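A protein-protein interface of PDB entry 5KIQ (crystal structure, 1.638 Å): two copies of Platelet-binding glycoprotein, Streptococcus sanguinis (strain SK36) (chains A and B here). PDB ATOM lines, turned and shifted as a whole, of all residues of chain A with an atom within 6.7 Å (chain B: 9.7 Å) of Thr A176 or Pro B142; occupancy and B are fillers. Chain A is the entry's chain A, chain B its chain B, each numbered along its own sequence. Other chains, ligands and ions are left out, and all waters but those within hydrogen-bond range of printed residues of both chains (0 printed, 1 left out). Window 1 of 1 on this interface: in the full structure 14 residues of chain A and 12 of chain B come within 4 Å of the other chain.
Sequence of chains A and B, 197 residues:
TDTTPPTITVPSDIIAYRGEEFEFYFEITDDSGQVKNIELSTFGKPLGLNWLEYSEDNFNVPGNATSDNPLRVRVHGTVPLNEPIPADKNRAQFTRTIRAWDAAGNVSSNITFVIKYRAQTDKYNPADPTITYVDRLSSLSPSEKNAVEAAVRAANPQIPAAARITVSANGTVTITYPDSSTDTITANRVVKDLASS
The side-chain amide nitrogen (ND2) of Asn B146 lies within hydrogen-bond range of the backbone carbonyl oxygen (O) of Ala A163 (2.9 Å). NH1 of Arg A164 lies close to OE1 of Glu B149 (2.9 Å). The guanidinium group (NH1) of Arg A164 sits at hydrogen-bond distance from the side-chain amide oxygen (OD1) of Asn B146 (2.9 Å).
Among the printed residues, merely in contact across the chains: Ala A162 with Pro B142 (3.9 Å), Ala A162 with Ser B143 (3.8 Å), Ala A162 with Asn B146 (3.5 Å), Arg A164 with Lys B145 (3.6 Å), Thr A176 with Pro B142 (3.6 Å), Tyr A177 with Pro B142 (3.3 Å), Pro A178 with Pro B142 (3.9 Å) and Ser A180 with Pro B142 (3.9 Å).
No position is printed for both chains. Of the 11 pairs that touch across the chains among the printed residues, none has its exchanged pair printed and touching as well.
The backbone carbonyl oxygen (O) of Arg A164 is in hydrogen-bond range of the backbone NH (N) of Thr A176. OH of Tyr A177 sits close to OD2 of Asp A183, 2.8 Å away.
Printed residues of chain B that touch a printed residue of chain A: Pro B142, Ser B143, Lys B145, Asn B146 and Glu B149. Hydrophobic or aromatic side chains of chain B within 4 Å of the printed part of chain A: Pro B142. Of the 15 printed residues of chain A, 7 touch a printed residue of chain B. Hydrophobic or aromatic side chains of chain A that line the printed part of chain B: Ala A162. Along chain A the printed residues that touch a printed residue of chain B span positions 162 to 180. Among the printed residues, Asp or Glu carboxylates within 4 Å of a Lys or Arg side-chain nitrogen of the other chain: Arg A164 with Glu B149 (2.9 Å).
Thr A176 touches one residue of chain B. Pro B142 touches just these residues of chain A: Ala A162, Thr A176, Tyr A177, Pro A178 and Ser A180. Ala A163 touches just one residue of chain B: Asn B146. Ser A180 touches just one residue of chain B: Pro B142. Printed residues of chain A within 4 Å of Ser B143: Ala A162 (3.8 Å). Printed residues of chain A within 4 Å of Glu B149: Arg A164 (2.9 Å). Leu B140 touches none of the printed residues of chain A. Val B148 touches none of the printed residues of chain A. The nearest residue of chain B that does not touch Thr A176 is Ser B143 (6.4 Å). The nearest residue of chain A that does not touch Pro B142 is Arg A164 (4.1 Å).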
ATOM      1  N   ALA A 162     -22.058  24.145  12.563  1.00  0.00           N
ATOM      2  CA  ALA A 162     -22.305  22.855  13.167  1.00  0.00           C
ATOM      3  C   ALA A 162     -21.177  21.852  12.879  1.00  0.00           C
ATOM      4  O   ALA A 162     -21.222  20.737  13.367  1.00  0.00           O
ATOM      5  CB  ALA A 162     -23.640  22.299  12.698  1.00  0.00           C
ATOM      6  N   ALA A 163     -20.184  22.226  12.072  1.00  0.00           N
ATOM      7  CA  ALA A 163     -19.026  21.351  11.898  1.00  0.00           C
ATOM      8  C   ALA A 163     -18.226  21.396  13.195  1.00  0.00           C
ATOM      9  O   ALA A 163     -18.157  22.446  13.840  1.00  0.00           O
ATOM     10  CB  ALA A 163     -18.154  21.792  10.734  1.00  0.00           C
ATOM     11  N   ARG A 164     -17.627  20.266  13.545  1.00  0.00           N
ATOM     12  CA  ARG A 164     -16.829  20.160  14.764  1.00  0.00           C
ATOM     13  C   ARG A 164     -15.340  20.072  14.443  1.00  0.00           C
ATOM     14  O   ARG A 164     -14.889  19.235  13.681  1.00  0.00           O
ATOM     15  CB  ARG A 164     -17.266  18.957  15.581  1.00  0.00           C
ATOM     16  CG  ARG A 164     -16.554  18.869  16.961  1.00  0.00           C
ATOM     17  CD  ARG A 164     -17.453  18.233  17.935  1.00  0.00           C
ATOM     18  NE  ARG A 164     -16.832  18.132  19.260  1.00  0.00           N
ATOM     19  CZ  ARG A 164     -16.897  19.094  20.167  1.00  0.00           C
ATOM     20  NH1 ARG A 164     -17.552  20.218  19.913  1.00  0.00           N
ATOM     21  NH2 ARG A 164     -16.304  18.919  21.344  1.00  0.00           N
ATOM     22  N   ILE A 165     -14.550  20.935  15.081  1.00  0.00           N
ATOM     23  CA  ILE A 165     -13.115  20.954  14.849  1.00  0.00           C
ATOM     24  C   ILE A 165     -12.386  20.328  16.024  1.00  0.00           C
ATOM     25  O   ILE A 165     -12.605  20.761  17.145  1.00  0.00           O
ATOM     26  CB  ILE A 165     -12.614  22.396  14.668  1.00  0.00           C
ATOM     27  CG1 ILE A 165     -13.330  23.067  13.496  1.00  0.00           C
ATOM     28  CG2 ILE A 165     -11.109  22.419  14.448  1.00  0.00           C
ATOM     29  CD1 ILE A 165     -13.036  24.546  13.432  1.00  0.00           C
ATOM     30  N   THR A 166     -11.584  19.291  15.779  1.00  0.00           N
ATOM     31  CA  THR A 166     -10.771  18.656  16.849  1.00  0.00           C
ATOM     32  C   THR A 166      -9.276  18.761  16.550  1.00  0.00           C
ATOM     33  O   THR A 166      -8.868  18.987  15.394  1.00  0.00           O
ATOM     34  CB  THR A 166     -11.151  17.178  17.047  1.00  0.00           C
ATOM     35  OG1 THR A 166     -11.218  16.538  15.769  1.00  0.00           O
ATOM     36  CG2 THR A 166     -12.513  17.072  17.685  1.00  0.00           C
ATOM     37  N   THR A 174      -8.552  17.891  12.697  1.00  0.00           N
ATOM     38  CA  THR A 174      -9.683  17.291  11.947  1.00  0.00           C
ATOM     39  C   THR A 174     -10.917  18.187  11.951  1.00  0.00           C
ATOM     40  O   THR A 174     -11.375  18.637  13.013  1.00  0.00           O
ATOM     41  CB  THR A 174     -10.102  15.955  12.538  1.00  0.00           C
ATOM     42  OG1 THR A 174      -8.948  15.123  12.719  1.00  0.00           O
ATOM     43  CG2 THR A 174     -11.155  15.275  11.630  1.00  0.00           C
ATOM     44  N   ILE A 175     -11.477  18.425  10.765  1.00  0.00           N
ATOM     45  CA  ILE A 175     -12.730  19.154  10.653  1.00  0.00           C
ATOM     46  C   ILE A 175     -13.792  18.106  10.310  1.00  0.00           C
ATOM     47  O   ILE A 175     -13.670  17.448   9.288  1.00  0.00           O
ATOM     48  CB  ILE A 175     -12.656  20.264   9.588  1.00  0.00           C
ATOM     49  CG1 ILE A 175     -11.548  21.283   9.972  1.00  0.00           C
ATOM     50  CG2 ILE A 175     -14.012  20.934   9.438  1.00  0.00           C
ATOM     51  CD1 ILE A 175     -11.211  22.248   8.858  1.00  0.00           C
ATOM     52  N   THR A 176     -14.753  17.880  11.205  1.00  0.00           N
ATOM     53  CA  THR A 176     -15.844  16.927  10.924  1.00  0.00           C
ATOM     54  C   THR A 176     -17.148  17.652  10.602  1.00  0.00           C
ATOM     55  O   THR A 176     -17.757  18.307  11.442  1.00  0.00           O
ATOM     56  CB  THR A 176     -16.079  15.939  12.082  1.00  0.00           C
ATOM     57  OG1 THR A 176     -14.859  15.230  12.349  1.00  0.00           O
ATOM     58  CG2 THR A 176     -17.191  14.907  11.668  1.00  0.00           C
ATOM     59  N   TYR A 177     -17.580  17.565   9.348  1.00  0.00           N
ATOM     60  CA  TYR A 177     -18.778  18.301   8.952  1.00  0.00           C
ATOM     61  C   TYR A 177     -20.051  17.639   9.525  1.00  0.00           C
ATOM     62  O   TYR A 177     -20.001  16.492   9.973  1.00  0.00           O
ATOM     63  CB  TYR A 177     -18.811  18.403   7.424  1.00  0.00           C
ATOM     64  CG  TYR A 177     -17.597  19.122   6.905  1.00  0.00           C
ATOM     65  CD1 TYR A 177     -17.488  20.503   7.020  1.00  0.00           C
ATOM     66  CD2 TYR A 177     -16.529  18.416   6.362  1.00  0.00           C
ATOM     67  CE1 TYR A 177     -16.356  21.165   6.567  1.00  0.00           C
ATOM     68  CE2 TYR A 177     -15.381  19.084   5.916  1.00  0.00           C
ATOM     69  CZ  TYR A 177     -15.304  20.448   6.027  1.00  0.00           C
ATOM     70  OH  TYR A 177     -14.167  21.113   5.588  1.00  0.00           O
ATOM     71  N   PRO A 178     -21.184  18.366   9.545  1.00  0.00           N
ATOM     72  CA  PRO A 178     -22.421  17.811  10.115  1.00  0.00           C
ATOM     73  C   PRO A 178     -22.842  16.455   9.558  1.00  0.00           C
ATOM     74  O   PRO A 178     -23.497  15.696  10.282  1.00  0.00           O
ATOM     75  CB  PRO A 178     -23.453  18.884   9.765  1.00  0.00           C
ATOM     76  CG  PRO A 178     -22.630  20.161   9.847  1.00  0.00           C
ATOM     77  CD  PRO A 178     -21.370  19.770   9.138  1.00  0.00           C
ATOM     78  N   ASP A 179     -22.473  16.142   8.310  1.00  0.00           N
ATOM     79  CA  ASP A 179     -22.772  14.820   7.744  1.00  0.00           C
ATOM     80  C   ASP A 179     -21.708  13.758   8.009  1.00  0.00           C
ATOM     81  O   ASP A 179     -21.685  12.716   7.362  1.00  0.00           O
ATOM     82  CB  ASP A 179     -23.023  14.940   6.213  1.00  0.00           C
ATOM     83  CG  ASP A 179     -21.732  15.199   5.417  1.00  0.00           C
ATOM     84  OD1 ASP A 179     -20.688  15.543   6.014  1.00  0.00           O
ATOM     85  OD2 ASP A 179     -21.732  15.068   4.181  1.00  0.00           O
ATOM     86  N   SER A 180     -20.829  14.031   8.985  1.00  0.00           N
ATOM     87  CA  SER A 180     -19.727  13.164   9.370  1.00  0.00           C
ATOM     88  C   SER A 180     -18.582  12.970   8.366  1.00  0.00           C
ATOM     89  O   SER A 180     -17.672  12.179   8.637  1.00  0.00           O
ATOM     90  CB  SER A 180     -20.272  11.810   9.795  1.00  0.00           C
ATOM     91  OG  SER A 180     -20.901  11.971  11.066  1.00  0.00           O
ATOM     92  N   SER A 181     -18.572  13.721   7.257  1.00  0.00           N
ATOM     93  CA  SER A 181     -17.411  13.688   6.348  1.00  0.00           C
ATOM     94  C   SER A 181     -16.344  14.626   6.937  1.00  0.00           C
ATOM     95  O   SER A 181     -16.669  15.425   7.818  1.00  0.00           O
ATOM     96  CB  SER A 181     -17.779  14.082   4.894  1.00  0.00           C
ATOM     97  OG  SER A 181     -18.154  15.448   4.734  1.00  0.00           O
ATOM     98  N   THR A 182     -15.084  14.496   6.503  1.00  0.00           N
ATOM     99  CA  THR A 182     -13.968  15.222   7.159  1.00  0.00           C
ATOM    100  C   THR A 182     -12.929  15.872   6.232  1.00  0.00           C
ATOM    101  O   THR A 182     -12.818  15.542   5.058  1.00  0.00           O
ATOM    102  CB  THR A 182     -13.164  14.299   8.101  1.00  0.00           C
ATOM    103  OG1 THR A 182     -12.463  13.314   7.326  1.00  0.00           O
ATOM    104  CG2 THR A 182     -14.063  13.613   9.142  1.00  0.00           C
ATOM    105  N   ASP A 183     -12.167  16.817   6.779  1.00  0.00           N
ATOM    106  CA  ASP A 183     -10.945  17.312   6.145  1.00  0.00           C
ATOM    107  C   ASP A 183      -9.867  17.277   7.254  1.00  0.00           C
ATOM    108  O   ASP A 183     -10.220  17.236   8.440  1.00  0.00           O
ATOM    109  CB  ASP A 183     -11.106  18.732   5.591  1.00  0.00           C
ATOM    110  CG  ASP A 183     -11.739  18.781   4.162  1.00  0.00           C
ATOM    111  OD1 ASP A 183     -11.580  17.874   3.320  1.00  0.00           O
ATOM    112  OD2 ASP A 183     -12.381  19.809   3.905  1.00  0.00           O
ATOM    113  N   THR B 132     -29.472  18.183  26.376  1.00  0.00           N
ATOM    114  CA  THR B 132     -29.483  18.141  24.912  1.00  0.00           C
ATOM    115  C   THR B 132     -30.178  16.878  24.418  1.00  0.00           C
ATOM    116  O   THR B 132     -29.782  15.768  24.782  1.00  0.00           O
ATOM    117  CB  THR B 132     -28.044  18.191  24.323  1.00  0.00           C
ATOM    118  OG1 THR B 132     -27.437  19.446  24.652  1.00  0.00           O
ATOM    119  CG2 THR B 132     -28.058  18.041  22.807  1.00  0.00           C
ATOM    120  N   VAL B 134     -30.950  14.155  21.630  1.00  0.00           N
ATOM    121  CA  VAL B 134     -30.181  13.611  20.523  1.00  0.00           C
ATOM    122  C   VAL B 134     -30.951  12.474  19.848  1.00  0.00           C
ATOM    123  O   VAL B 134     -31.946  11.984  20.386  1.00  0.00           O
ATOM    124  CB  VAL B 134     -28.799  13.110  21.002  1.00  0.00           C
ATOM    125  CG1 VAL B 134     -28.106  14.197  21.804  1.00  0.00           C
ATOM    126  CG2 VAL B 134     -28.931  11.862  21.858  1.00  0.00           C
ATOM    127  N   ARG B 136     -29.454   9.416  18.558  1.00  0.00           N
ATOM    128  CA  ARG B 136     -28.911   8.159  19.056  1.00  0.00           C
ATOM    129  C   ARG B 136     -28.060   8.389  20.302  1.00  0.00           C
ATOM    130  O   ARG B 136     -26.973   8.950  20.203  1.00  0.00           O
ATOM    131  CB  ARG B 136     -28.065   7.468  17.987  1.00  0.00           C
ATOM    132  CG  ARG B 136     -28.853   6.763  16.902  1.00  0.00           C
ATOM    133  CD  ARG B 136     -27.909   6.026  15.959  1.00  0.00           C
ATOM    134  NE  ARG B 136     -27.171   6.948  15.096  1.00  0.00           N
ATOM    135  CZ  ARG B 136     -25.986   6.682  14.551  1.00  0.00           C
ATOM    136  NH1 ARG B 136     -25.387   5.520  14.786  1.00  0.00           N
ATOM    137  NH2 ARG B 136     -25.392   7.584  13.777  1.00  0.00           N
ATOM    138  N   SER B 139     -24.453   7.322  19.812  1.00  0.00           N
ATOM    139  CA  SER B 139     -23.627   7.930  18.780  1.00  0.00           C
ATOM    140  C   SER B 139     -24.092   9.337  18.437  1.00  0.00           C
ATOM    141  O   SER B 139     -24.902   9.539  17.536  1.00  0.00           O
ATOM    142  CB  SER B 139     -23.624   7.073  17.515  1.00  0.00           C
ATOM    143  OG  SER B 139     -23.036   7.789  16.442  1.00  0.00           O
ATOM    144  N   LEU B 140     -23.564  10.314  19.156  1.00  0.00           N
ATOM    145  CA  LEU B 140     -23.887  11.701  18.906  1.00  0.00           C
ATOM    146  C   LEU B 140     -23.316  12.171  17.570  1.00  0.00           C
ATOM    147  O   LEU B 140     -22.258  11.718  17.143  1.00  0.00           O
ATOM    148  CB  LEU B 140     -23.342  12.574  20.048  1.00  0.00           C
ATOM    149  CG  LEU B 140     -24.306  12.921  21.187  1.00  0.00           C
ATOM    150  CD1 LEU B 140     -24.719  11.684  21.972  1.00  0.00           C
ATOM    151  CD2 LEU B 140     -23.637  13.953  22.091  1.00  0.00           C
ATOM    152  N   SER B 141     -24.014  13.088  16.921  1.00  0.00           N
ATOM    153  CA  SER B 141     -23.529  13.697  15.681  1.00  0.00           C
ATOM    154  C   SER B 141     -22.571  14.852  15.998  1.00  0.00           C
ATOM    155  O   SER B 141     -22.515  15.285  17.144  1.00  0.00           O
ATOM    156  CB  SER B 141     -24.717  14.197  14.852  1.00  0.00           C
ATOM    157  OG  SER B 141     -25.387  15.251  15.529  1.00  0.00           O
ATOM    158  N   PRO B 142     -21.824  15.361  14.992  1.00  0.00           N
ATOM    159  CA  PRO B 142     -20.991  16.552  15.230  1.00  0.00           C
ATOM    160  C   PRO B 142     -21.792  17.734  15.768  1.00  0.00           C
ATOM    161  O   PRO B 142     -21.349  18.436  16.679  1.00  0.00           O
ATOM    162  CB  PRO B 142     -20.417  16.876  13.839  1.00  0.00           C
ATOM    163  CG  PRO B 142     -20.443  15.610  13.122  1.00  0.00           C
ATOM    164  CD  PRO B 142     -21.626  14.830  13.626  1.00  0.00           C
ATOM    165  N   SER B 143     -22.975  17.956  15.209  1.00  0.00           N
ATOM    166  CA  SER B 143     -23.824  19.047  15.624  1.00  0.00           C
ATOM    167  C   SER B 143     -24.255  18.895  17.095  1.00  0.00           C
ATOM    168  O   SER B 143     -24.249  19.868  17.854  1.00  0.00           O
ATOM    169  CB  SER B 143     -25.042  19.121  14.680  1.00  0.00           C
ATOM    170  OG  SER B 143     -25.935  20.142  15.075  1.00  0.00           O
ATOM    171  N   GLU B 144     -24.605  17.671  17.494  1.00  0.00           N
ATOM    172  CA  GLU B 144     -25.033  17.400  18.855  1.00  0.00           C
ATOM    173  C   GLU B 144     -23.862  17.591  19.834  1.00  0.00           C
ATOM    174  O   GLU B 144     -24.074  18.059  20.948  1.00  0.00           O
ATOM    175  CB  GLU B 144     -25.599  15.987  18.995  1.00  0.00           C
ATOM    176  CG  GLU B 144     -26.978  15.869  18.289  1.00  0.00           C
ATOM    177  CD  GLU B 144     -27.428  14.437  17.997  1.00  0.00           C
ATOM    178  OE1 GLU B 144     -26.586  13.510  18.058  1.00  0.00           O
ATOM    179  OE2 GLU B 144     -28.638  14.252  17.682  1.00  0.00           O
ATOM    180  N   LYS B 145     -22.650  17.226  19.409  1.00  0.00           N
ATOM    181  CA  LYS B 145     -21.470  17.427  20.265  1.00  0.00           C
ATOM    182  C   LYS B 145     -21.169  18.891  20.416  1.00  0.00           C
ATOM    183  O   LYS B 145     -20.834  19.339  21.511  1.00  0.00           O
ATOM    184  CB  LYS B 145     -20.253  16.706  19.704  1.00  0.00           C
ATOM    185  CG  LYS B 145     -20.346  15.208  19.826  1.00  0.00           C
ATOM    186  CD  LYS B 145     -19.097  14.520  19.306  1.00  0.00           C
ATOM    187  CE  LYS B 145     -19.322  13.014  19.267  1.00  0.00           C
ATOM    188  NZ  LYS B 145     -18.308  12.265  18.470  1.00  0.00           N
ATOM    189  N   ASN B 146     -21.265  19.640  19.318  1.00  0.00           N
ATOM    190  CA  ASN B 146     -21.104  21.079  19.387  1.00  0.00           C
ATOM    191  C   ASN B 146     -22.122  21.674  20.351  1.00  0.00           C
ATOM    192  O   ASN B 146     -21.773  22.562  21.137  1.00  0.00           O
ATOM    193  CB  ASN B 146     -21.267  21.742  18.017  1.00  0.00           C
ATOM    194  CG  ASN B 146     -19.967  21.868  17.247  1.00  0.00           C
ATOM    195  OD1 ASN B 146     -18.935  21.322  17.622  1.00  0.00           O
ATOM    196  ND2 ASN B 146     -20.031  22.580  16.112  1.00  0.00           N
ATOM    197  N   ALA B 147     -23.365  21.170  20.318  1.00  0.00           N
ATOM    198  CA  ALA B 147     -24.410  21.704  21.201  1.00  0.00           C
ATOM    199  C   ALA B 147     -24.147  21.367  22.667  1.00  0.00           C
ATOM    200  O   ALA B 147     -24.344  22.213  23.534  1.00  0.00           O
ATOM    201  CB  ALA B 147     -25.769  21.194  20.808  1.00  0.00           C
ATOM    202  N   VAL B 148     -23.760  20.119  22.937  1.00  0.00           N
ATOM    203  CA  VAL B 148     -23.373  19.721  24.291  1.00  0.00           C
ATOM    204  C   VAL B 148     -22.222  20.598  24.799  1.00  0.00           C
ATOM    205  O   VAL B 148     -22.328  21.151  25.903  1.00  0.00           O
ATOM    206  CB  VAL B 148     -22.973  18.245  24.353  1.00  0.00           C
ATOM    207  CG1 VAL B 148     -22.303  17.948  25.670  1.00  0.00           C
ATOM    208  CG2 VAL B 148     -24.204  17.356  24.187  1.00  0.00           C
ATOM    209  N   GLU B 149     -21.153  20.766  24.006  1.00  0.00           N
ATOM    210  CA  GLU B 149     -20.000  21.580  24.477  1.00  0.00           C
ATOM    211  C   GLU B 149     -20.491  23.000  24.807  1.00  0.00           C
ATOM    212  O   GLU B 149     -20.134  23.550  25.840  1.00  0.00           O
ATOM    213  CB  GLU B 149     -18.823  21.630  23.452  1.00  0.00           C
ATOM    214  CG  GLU B 149     -17.530  22.429  23.948  1.00  0.00           C
ATOM    215  CD  GLU B 149     -16.358  22.572  22.904  1.00  0.00           C
ATOM    216  OE1 GLU B 149     -16.310  21.905  21.852  1.00  0.00           O
ATOM    217  OE2 GLU B 149     -15.429  23.379  23.106  1.00  0.00           O
ATOM    218  N   ALA B 150     -21.333  23.567  23.946  1.00  0.00           N
ATOM    219  CA  ALA B 150     -21.893  24.903  24.168  1.00  0.00           C
ATOM    220  C   ALA B 150     -22.776  24.967  25.425  1.00  0.00           C
ATOM    221  O   ALA B 150     -22.775  25.968  26.128  1.00  0.00           O
ATOM    222  CB  ALA B 150     -22.686  25.353  22.938  1.00  0.00           C
ATOM    223  N   VAL B 167     -16.273  16.041  24.144  1.00  0.00           N
ATOM    224  CA  VAL B 167     -17.510  15.275  24.238  1.00  0.00           C
ATOM    225  C   VAL B 167     -17.267  13.958  23.523  1.00  0.00           C
ATOM    226  O   VAL B 167     -16.732  13.945  22.408  1.00  0.00           O
ATOM    227  CB  VAL B 167     -18.728  16.020  23.609  1.00  0.00           C
ATOM    228  CG1 VAL B 167     -20.034  15.221  23.837  1.00  0.00           C
ATOM    229  CG2 VAL B 167     -18.854  17.451  24.157  1.00  0.00           C
ATOM    230  N   SER B 168     -17.635  12.851  24.165  1.00  0.00           N
ATOM    231  CA  SER B 168     -17.454  11.532  23.565  1.00  0.00           C
ATOM    232  C   SER B 168     -18.673  11.153  22.731  1.00  0.00           C
ATOM    233  O   SER B 168     -19.685  11.854  22.736  1.00  0.00           O
ATOM    234  CB  SER B 168     -17.227  10.454  24.631  1.00  0.00           C
ATOM    235  OG  SER B 168     -18.441  10.142  25.303  1.00  0.00           O
ATOM    236  N   ALA B 169     -18.565  10.006  22.074  1.00  0.00           N
ATOM    237  CA  ALA B 169     -19.631   9.434  21.251  1.00  0.00           C
ATOM    238  C   ALA B 169     -20.982   9.307  21.971  1.00  0.00           C
ATOM    239  O   ALA B 169     -22.036   9.484  21.346  1.00  0.00           O
ATOM    240  CB  ALA B 169     -19.190   8.091  20.741  1.00  0.00           C
